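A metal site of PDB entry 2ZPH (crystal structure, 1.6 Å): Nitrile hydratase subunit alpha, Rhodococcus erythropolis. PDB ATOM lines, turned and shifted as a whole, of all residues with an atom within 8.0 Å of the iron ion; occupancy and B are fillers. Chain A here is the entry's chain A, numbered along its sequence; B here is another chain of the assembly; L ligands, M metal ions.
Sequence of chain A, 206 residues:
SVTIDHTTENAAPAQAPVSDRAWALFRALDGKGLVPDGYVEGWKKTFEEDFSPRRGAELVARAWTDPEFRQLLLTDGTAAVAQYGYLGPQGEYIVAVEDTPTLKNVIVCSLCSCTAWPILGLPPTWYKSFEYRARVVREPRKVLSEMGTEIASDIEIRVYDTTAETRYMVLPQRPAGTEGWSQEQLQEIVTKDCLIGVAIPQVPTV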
ATOM      1  N   GLN A  90      14.512 -15.404  33.223  1.00  0.00           N
ATOM      2  CA  GLN A  90      13.945 -15.371  31.870  1.00  0.00           C
ATOM      3  C   GLN A  90      14.990 -14.991  30.815  1.00  0.00           C
ATOM      4  O   GLN A  90      14.676 -14.375  29.792  1.00  0.00           O
ATOM      5  CB  GLN A  90      12.726 -14.442  31.824  1.00  0.00           C
ATOM      6  CG  GLN A  90      11.553 -14.966  32.670  1.00  0.00           C
ATOM      7  CD  GLN A  90      11.069 -16.330  32.208  1.00  0.00           C
ATOM      8  OE1 GLN A  90      10.661 -16.493  31.052  1.00  0.00           O
ATOM      9  NE2 GLN A  90      11.150 -17.316  33.092  1.00  0.00           N
ATOM     10  N   VAL A 108       8.141 -13.407  19.123  1.00  0.00           N
ATOM     11  CA  VAL A 108       6.876 -13.264  19.847  1.00  0.00           C
ATOM     12  C   VAL A 108       6.776 -14.361  20.904  1.00  0.00           C
ATOM     13  O   VAL A 108       7.535 -15.325  20.862  1.00  0.00           O
ATOM     14  CB  VAL A 108       5.673 -13.397  18.874  1.00  0.00           C
ATOM     15  CG1 VAL A 108       5.620 -14.799  18.241  1.00  0.00           C
ATOM     16  CG2 VAL A 108       4.351 -13.040  19.566  1.00  0.00           C
ATOM     17  N   CYS A 109       5.848 -14.193  21.843  1.00  0.00           N
ATOM     18  CA  CYS A 109       5.400 -15.324  22.653  1.00  0.00           C
ATOM     19  C   CYS A 109       3.891 -15.413  22.452  1.00  0.00           C
ATOM     20  O   CYS A 109       3.129 -14.710  23.114  1.00  0.00           O
ATOM     21  CB  CYS A 109       5.726 -15.144  24.142  1.00  0.00           C
ATOM     22  SG  CYS A 109       5.059 -16.501  25.179  1.00  0.00           S
ATOM     23  N   SER A 110       3.439 -16.256  21.524  1.00  0.00           N
ATOM     24  CA  SER A 110       2.014 -16.294  21.221  1.00  0.00           C
ATOM     25  C   SER A 110       1.176 -16.786  22.412  1.00  0.00           C
ATOM     26  O   SER A 110       0.009 -16.414  22.546  1.00  0.00           O
ATOM     27  CB  SER A 110       1.738 -17.155  19.986  1.00  0.00           C
ATOM     28  OG  SER A 110       1.947 -18.523  20.267  1.00  0.00           O
ATOM     29  N   LEU A 111       1.777 -17.601  23.275  1.00  0.00           N
ATOM     30  CA  LEU A 111       1.060 -18.226  24.382  1.00  0.00           C
ATOM     31  C   LEU A 111       1.009 -17.384  25.647  1.00  0.00           C
ATOM     32  O   LEU A 111       0.201 -17.673  26.539  1.00  0.00           O
ATOM     33  CB  LEU A 111       1.658 -19.611  24.703  1.00  0.00           C
ATOM     34  CG  LEU A 111       1.561 -20.648  23.582  1.00  0.00           C
ATOM     35  CD1 LEU A 111       2.431 -21.856  23.931  1.00  0.00           C
ATOM     36  CD2 LEU A 111       0.110 -21.070  23.306  1.00  0.00           C
ATOM     37  N   CSD A 112       1.839 -16.345  25.728  1.00  0.00           N
ATOM     38  CA  CSD A 112       1.876 -15.455  26.915  1.00  0.00           C
ATOM     39  CB  CSD A 112       2.292 -16.203  28.193  1.00  0.00           C
ATOM     40  SG  CSD A 112       3.759 -17.175  28.011  1.00  0.00           S
ATOM     41  C   CSD A 112       2.706 -14.192  26.704  1.00  0.00           C
ATOM     42  O   CSD A 112       2.167 -13.168  26.241  1.00  0.00           O
ATOM     43  OD1 CSD A 112       4.006 -17.708  29.640  1.00  0.00           O
ATOM     44  OD2 CSD A 112       3.415 -18.362  27.141  1.00  0.00           O
ATOM     45  N   SER A 113       3.991 -14.223  27.044  1.00  0.00           N
ATOM     46  CA  SER A 113       4.771 -12.980  26.915  1.00  0.00           C
ATOM     47  C   SER A 113       6.266 -13.231  26.936  1.00  0.00           C
ATOM     48  O   SER A 113       7.062 -12.266  26.969  1.00  0.00           O
ATOM     49  CB  SER A 113       4.413 -12.010  28.030  1.00  0.00           C
ATOM     50  OG  SER A 113       4.817 -12.515  29.299  1.00  0.00           O
ATOM     51  N   CSO A 114       6.651 -14.505  26.888  1.00  0.00           N
ATOM     52  CA  CSO A 114       8.045 -14.912  26.995  1.00  0.00           C
ATOM     53  CB  CSO A 114       8.219 -16.385  26.617  1.00  0.00           C
ATOM     54  SG  CSO A 114       6.915 -17.304  27.473  1.00  0.00           S
ATOM     55  C   CSO A 114       8.994 -13.990  26.230  1.00  0.00           C
ATOM     56  O   CSO A 114       8.838 -13.752  25.024  1.00  0.00           O
ATOM     57  OD  CSO A 114       7.447 -17.473  29.123  1.00  0.00           O
ATOM     58  N   THR A 115       9.992 -13.479  26.966  1.00  0.00           N
ATOM     59  CA  THR A 115      10.921 -12.449  26.506  1.00  0.00           C
ATOM     60  C   THR A 115      12.237 -12.626  27.233  1.00  0.00           C
ATOM     61  O   THR A 115      12.230 -12.979  28.413  1.00  0.00           O
ATOM     62  CB  THR A 115      10.343 -11.082  26.874  1.00  0.00           C
ATOM     63  OG1 THR A 115       9.186 -10.823  26.068  1.00  0.00           O
ATOM     64  CG2 THR A 115      11.362  -9.954  26.711  1.00  0.00           C
ATOM     65  N   TRP A 117      14.151 -11.126  29.283  1.00  0.00           N
ATOM     66  CA  TRP A 117      14.096  -9.956  30.168  1.00  0.00           C
ATOM     67  C   TRP A 117      15.417  -9.211  30.415  1.00  0.00           C
ATOM     68  O   TRP A 117      15.442  -7.986  30.363  1.00  0.00           O
ATOM     69  CB  TRP A 117      13.553 -10.337  31.541  1.00  0.00           C
ATOM     70  CG  TRP A 117      12.113 -10.735  31.612  1.00  0.00           C
ATOM     71  CD1 TRP A 117      11.159 -10.626  30.655  1.00  0.00           C
ATOM     72  CD2 TRP A 117      11.474 -11.302  32.763  1.00  0.00           C
ATOM     73  NE1 TRP A 117       9.941 -11.090  31.129  1.00  0.00           N
ATOM     74  CE2 TRP A 117      10.116 -11.512  32.427  1.00  0.00           C
ATOM     75  CE3 TRP A 117      11.914 -11.621  34.058  1.00  0.00           C
ATOM     76  CZ2 TRP A 117       9.207 -12.058  33.344  1.00  0.00           C
ATOM     77  CZ3 TRP A 117      11.015 -12.160  34.955  1.00  0.00           C
ATOM     78  CH2 TRP A 117       9.678 -12.372  34.599  1.00  0.00           C
ATOM     79  N   PRO A 123       8.764  -7.180  28.707  1.00  0.00           N
ATOM     80  CA  PRO A 123       8.040  -6.901  27.479  1.00  0.00           C
ATOM     81  C   PRO A 123       7.115  -5.695  27.627  1.00  0.00           C
ATOM     82  O   PRO A 123       6.538  -5.487  28.702  1.00  0.00           O
ATOM     83  CB  PRO A 123       7.217  -8.172  27.248  1.00  0.00           C
ATOM     84  CG  PRO A 123       7.117  -8.824  28.601  1.00  0.00           C
ATOM     85  CD  PRO A 123       8.437  -8.512  29.256  1.00  0.00           C
ATOM     86  N   TYR A 127       3.607  -5.922  23.009  1.00  0.00           N
ATOM     87  CA  TYR A 127       4.157  -7.251  22.679  1.00  0.00           C
ATOM     88  C   TYR A 127       3.299  -8.318  23.341  1.00  0.00           C
ATOM     89  O   TYR A 127       3.161  -9.430  22.821  1.00  0.00           O
ATOM     90  CB  TYR A 127       5.584  -7.303  23.189  1.00  0.00           C
ATOM     91  CG  TYR A 127       6.308  -8.626  23.050  1.00  0.00           C
ATOM     92  CD1 TYR A 127       6.223  -9.591  24.066  1.00  0.00           C
ATOM     93  CD2 TYR A 127       7.130  -8.878  21.959  1.00  0.00           C
ATOM     94  CE1 TYR A 127       6.927 -10.784  23.973  1.00  0.00           C
ATOM     95  CE2 TYR A 127       7.824 -10.074  21.846  1.00  0.00           C
ATOM     96  CZ  TYR A 127       7.729 -11.021  22.849  1.00  0.00           C
ATOM     97  OH  TYR A 127       8.456 -12.190  22.756  1.00  0.00           O
ATOM     98  N   LYS A 128       2.761  -7.984  24.504  1.00  0.00           N
ATOM     99  CA  LYS A 128       1.874  -8.873  25.249  1.00  0.00           C
ATOM    100  C   LYS A 128       0.419  -8.783  24.777  1.00  0.00           C
ATOM    101  O   LYS A 128      -0.443  -9.523  25.254  1.00  0.00           O
ATOM    102  CB  LYS A 128       1.957  -8.525  26.752  1.00  0.00           C
ATOM    103  CG  LYS A 128       3.365  -8.605  27.286  1.00  0.00           C
ATOM    104  CD  LYS A 128       3.449  -8.120  28.733  1.00  0.00           C
ATOM    105  CE  LYS A 128       3.385  -6.611  28.852  1.00  0.00           C
ATOM    106  NZ  LYS A 128       3.871  -6.143  30.188  1.00  0.00           N
ATOM    107  N   ARG A 133       0.156 -11.174  19.589  1.00  0.00           N
ATOM    108  CA  ARG A 133       0.220 -12.615  19.841  1.00  0.00           C
ATOM    109  C   ARG A 133      -0.547 -13.426  18.795  1.00  0.00           C
ATOM    110  O   ARG A 133      -0.107 -14.503  18.382  1.00  0.00           O
ATOM    111  CB  ARG A 133      -0.326 -12.899  21.262  1.00  0.00           C
ATOM    112  CG  ARG A 133       0.634 -12.414  22.361  1.00  0.00           C
ATOM    113  CD  ARG A 133       0.077 -12.645  23.795  1.00  0.00           C
ATOM    114  NE  ARG A 133      -0.457 -13.996  23.956  1.00  0.00           N
ATOM    115  CZ  ARG A 133      -1.358 -14.348  24.871  1.00  0.00           C
ATOM    116  NH1 ARG A 133      -1.810 -13.461  25.753  1.00  0.00           N
ATOM    117  NH2 ARG A 133      -1.815 -15.607  24.907  1.00  0.00           N
ATOM    118  N   ASP A 161       8.573 -18.145  17.747  1.00  0.00           N
ATOM    119  CA  ASP A 161       7.587 -18.182  18.814  1.00  0.00           C
ATOM    120  C   ASP A 161       8.254 -18.777  20.049  1.00  0.00           C
ATOM    121  O   ASP A 161       8.729 -19.921  20.030  1.00  0.00           O
ATOM    122  CB  ASP A 161       6.384 -19.010  18.361  1.00  0.00           C
ATOM    123  CG  ASP A 161       5.149 -18.785  19.210  1.00  0.00           C
ATOM    124  OD1 ASP A 161       5.269 -18.125  20.274  1.00  0.00           O
ATOM    125  OD2 ASP A 161       4.066 -19.281  18.823  1.00  0.00           O
ATOM    126  N   THR A 162       8.304 -17.993  21.119  1.00  0.00           N
ATOM    127  CA  THR A 162       9.043 -18.331  22.328  1.00  0.00           C
ATOM    128  C   THR A 162       8.188 -19.237  23.221  1.00  0.00           C
ATOM    129  O   THR A 162       7.527 -18.777  24.160  1.00  0.00           O
ATOM    130  CB  THR A 162       9.448 -17.049  23.075  1.00  0.00           C
ATOM    131  OG1 THR A 162      10.116 -16.145  22.173  1.00  0.00           O
ATOM    132  CG2 THR A 162      10.388 -17.402  24.220  1.00  0.00           C
ATOM    133  N   THR A 163       8.207 -20.524  22.906  1.00  0.00           N
ATOM    134  CA  THR A 163       7.305 -21.502  23.512  1.00  0.00           C
ATOM    135  C   THR A 163       7.931 -22.361  24.590  1.00  0.00           C
ATOM    136  O   THR A 163       7.220 -23.141  25.250  1.00  0.00           O
ATOM    137  CB  THR A 163       6.718 -22.412  22.409  1.00  0.00           C
ATOM    138  OG1 THR A 163       7.798 -22.898  21.592  1.00  0.00           O
ATOM    139  CG2 THR A 163       5.735 -21.651  21.532  1.00  0.00           C
ATOM    140  N   ALA A 164       9.243 -22.255  24.768  1.00  0.00           N
ATOM    141  CA  ALA A 164       9.904 -23.060  25.816  1.00  0.00           C
ATOM    142  C   ALA A 164      10.874 -22.190  26.595  1.00  0.00           C
ATOM    143  O   ALA A 164      10.500 -21.094  27.024  1.00  0.00           O
ATOM    144  CB  ALA A 164      10.586 -24.292  25.213  1.00  0.00           C
ATOM    145  N   ARG A 167      15.456 -18.117  25.057  1.00  0.00           N
ATOM    146  CA  ARG A 167      15.082 -16.712  25.080  1.00  0.00           C
ATOM    147  C   ARG A 167      15.888 -16.042  23.990  1.00  0.00           C
ATOM    148  O   ARG A 167      17.113 -16.213  23.894  1.00  0.00           O
ATOM    149  CB  ARG A 167      15.358 -16.108  26.458  1.00  0.00           C
ATOM    150  CG  ARG A 167      14.440 -16.701  27.536  1.00  0.00           C
ATOM    151  CD  ARG A 167      13.000 -16.155  27.447  1.00  0.00           C
ATOM    152  NE  ARG A 167      12.119 -16.821  28.398  1.00  0.00           N
ATOM    153  CZ  ARG A 167      11.524 -17.997  28.168  1.00  0.00           C
ATOM    154  NH1 ARG A 167      11.695 -18.615  27.003  1.00  0.00           N
ATOM    155  NH2 ARG A 167      10.758 -18.556  29.103  1.00  0.00           N
ATOM    156  N   TYR B  37       4.911 -10.392  39.353  1.00  0.00           N
ATOM    157  CA  TYR B  37       6.167 -11.104  39.084  1.00  0.00           C
ATOM    158  C   TYR B  37       6.953 -11.338  40.382  1.00  0.00           C
ATOM    159  O   TYR B  37       7.506 -12.425  40.601  1.00  0.00           O
ATOM    160  CB  TYR B  37       7.053 -10.333  38.106  1.00  0.00           C
ATOM    161  CG  TYR B  37       6.670 -10.372  36.644  1.00  0.00           C
ATOM    162  CD1 TYR B  37       5.661 -11.208  36.149  1.00  0.00           C
ATOM    163  CD2 TYR B  37       7.370  -9.569  35.736  1.00  0.00           C
ATOM    164  CE1 TYR B  37       5.349 -11.200  34.777  1.00  0.00           C
ATOM    165  CE2 TYR B  37       7.084  -9.579  34.403  1.00  0.00           C
ATOM    166  CZ  TYR B  37       6.082 -10.396  33.922  1.00  0.00           C
ATOM    167  OH  TYR B  37       5.832 -10.373  32.553  1.00  0.00           O
ATOM    168  N   ARG B  56       2.094 -20.298  34.399  1.00  0.00           N
ATOM    169  CA  ARG B  56       1.543 -20.218  33.047  1.00  0.00           C
ATOM    170  C   ARG B  56       0.205 -20.952  32.986  1.00  0.00           C
ATOM    171  O   ARG B  56      -0.771 -20.429  32.461  1.00  0.00           O
ATOM    172  CB  ARG B  56       2.492 -20.850  32.038  1.00  0.00           C
ATOM    173  CG  ARG B  56       3.802 -20.120  31.928  1.00  0.00           C
ATOM    174  CD  ARG B  56       4.551 -20.539  30.655  1.00  0.00           C
ATOM    175  NE  ARG B  56       5.783 -19.764  30.560  1.00  0.00           N
ATOM    176  CZ  ARG B  56       6.943 -20.145  31.087  1.00  0.00           C
ATOM    177  NH1 ARG B  56       7.042 -21.309  31.702  1.00  0.00           N
ATOM    178  NH2 ARG B  56       8.011 -19.348  30.983  1.00  0.00           N
ATOM    179  N   TYR B  72      -2.855  -7.719  31.090  1.00  0.00           N
ATOM    180  CA  TYR B  72      -1.743  -8.614  31.358  1.00  0.00           C
ATOM    181  C   TYR B  72      -1.362  -8.780  32.840  1.00  0.00           C
ATOM    182  O   TYR B  72      -1.430  -9.892  33.388  1.00  0.00           O
ATOM    183  CB  TYR B  72      -0.502  -8.188  30.543  1.00  0.00           C
ATOM    184  CG  TYR B  72       0.657  -9.098  30.791  1.00  0.00           C
ATOM    185  CD1 TYR B  72       0.817 -10.271  30.046  1.00  0.00           C
ATOM    186  CD2 TYR B  72       1.589  -8.821  31.793  1.00  0.00           C
ATOM    187  CE1 TYR B  72       1.882 -11.137  30.282  1.00  0.00           C
ATOM    188  CE2 TYR B  72       2.651  -9.688  32.046  1.00  0.00           C
ATOM    189  CZ  TYR B  72       2.790 -10.833  31.287  1.00  0.00           C
ATOM    190  OH  TYR B  72       3.842 -11.691  31.539  1.00  0.00           O
ATOM    191  N   TYR B  76      -1.778 -12.119  36.119  1.00  0.00           N
ATOM    192  CA  TYR B  76      -0.771 -12.754  36.986  1.00  0.00           C
ATOM    193  C   TYR B  76      -1.038 -12.538  38.476  1.00  0.00           C
ATOM    194  O   TYR B  76      -0.746 -13.396  39.289  1.00  0.00           O
ATOM    195  CB  TYR B  76       0.671 -12.374  36.571  1.00  0.00           C
ATOM    196  CG  TYR B  76       0.942 -12.961  35.198  1.00  0.00           C
ATOM    197  CD1 TYR B  76       1.511 -14.220  35.054  1.00  0.00           C
ATOM    198  CD2 TYR B  76       0.485 -12.306  34.053  1.00  0.00           C
ATOM    199  CE1 TYR B  76       1.676 -14.801  33.766  1.00  0.00           C
ATOM    200  CE2 TYR B  76       0.636 -12.865  32.798  1.00  0.00           C
ATOM    201  CZ  TYR B  76       1.225 -14.114  32.654  1.00  0.00           C
ATOM    202  OH  TYR B  76       1.356 -14.616  31.381  1.00  0.00           O
ATOM    203  N   ARG B 141       3.167 -26.899  26.023  1.00  0.00           N
ATOM    204  CA  ARG B 141       3.827 -25.772  25.352  1.00  0.00           C
ATOM    205  C   ARG B 141       3.908 -26.010  23.845  1.00  0.00           C
ATOM    206  O   ARG B 141       4.930 -25.776  23.214  1.00  0.00           O
ATOM    207  CB  ARG B 141       5.202 -25.512  25.968  1.00  0.00           C
ATOM    208  CG  ARG B 141       5.117 -25.070  27.418  1.00  0.00           C
ATOM    209  CD  ARG B 141       4.278 -23.790  27.524  1.00  0.00           C
ATOM    210  NE  ARG B 141       4.964 -22.660  26.900  1.00  0.00           N
ATOM    211  CZ  ARG B 141       4.481 -21.416  26.890  1.00  0.00           C
ATOM    212  NH1 ARG B 141       3.274 -21.164  27.386  1.00  0.00           N
ATOM    213  NH2 ARG B 141       5.201 -20.429  26.370  1.00  0.00           N
HETATM  214  C1  LIG L   1       5.471 -15.248  29.391  1.00  0.00           C
HETATM  215  N1  LIG L   1       5.807 -15.332  31.319  1.00  0.00           N
HETATM  216  C2  LIG L   1       6.041 -15.476  32.749  1.00  0.00           C
HETATM  217  C3  LIG L   1       7.537 -15.578  32.998  1.00  0.00           C
HETATM  218  C4  LIG L   1       5.357 -16.737  33.245  1.00  0.00           C
HETATM  219  C5  LIG L   1       5.448 -14.243  33.424  1.00  0.00           C
HETATM  220 FE    FE M   1       5.284 -15.814  27.385  1.00  0.00          FE
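The guanidinium group of Arg 167 lies within hydrogen-bond range of OD of CSO 114 (3.5 Å). OD1 of CSD 112 is in salt-bridge range of the guanidinium group (NE) of Arg 56 of chain B. O of CSO 114 is in hydrogen-bond range of the side-chain hydroxyl (OH) of Tyr 127 (2.8 Å). OD2 of CSD 112 is in salt-bridge range of the guanidinium group (NH1) of Arg 141 of chain B (2.8 Å). The backbone NH (N) of Cys 109 is in hydrogen-bond range of the side-chain hydroxyl (OH) of Tyr 127 (3.4 Å). OD of CSO 114 is in hydrogen-bond range of NH2 of Arg 56 of chain B, 2.7 Å away. The backbone carbonyl oxygen (O) of Ser 113 is in hydrogen-bond range of the side-chain hydroxyl (OG1) of Thr 115. OG of Ser 113 lies within hydrogen-bond range of OH of Tyr 72 of chain B (2.6 Å).
Within 4 Å of the iron ion: Cys 109, CSD 112, Ser 113 and CSO 114. The nearest printed residue that does not touch the iron ion is Arg 141 of chain B (4.7 Å).
The iron ion is bound by N of CSO 114, N of Ser 113, SG of CSD 112, SG of CSO 114 and SG of Cys 109.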
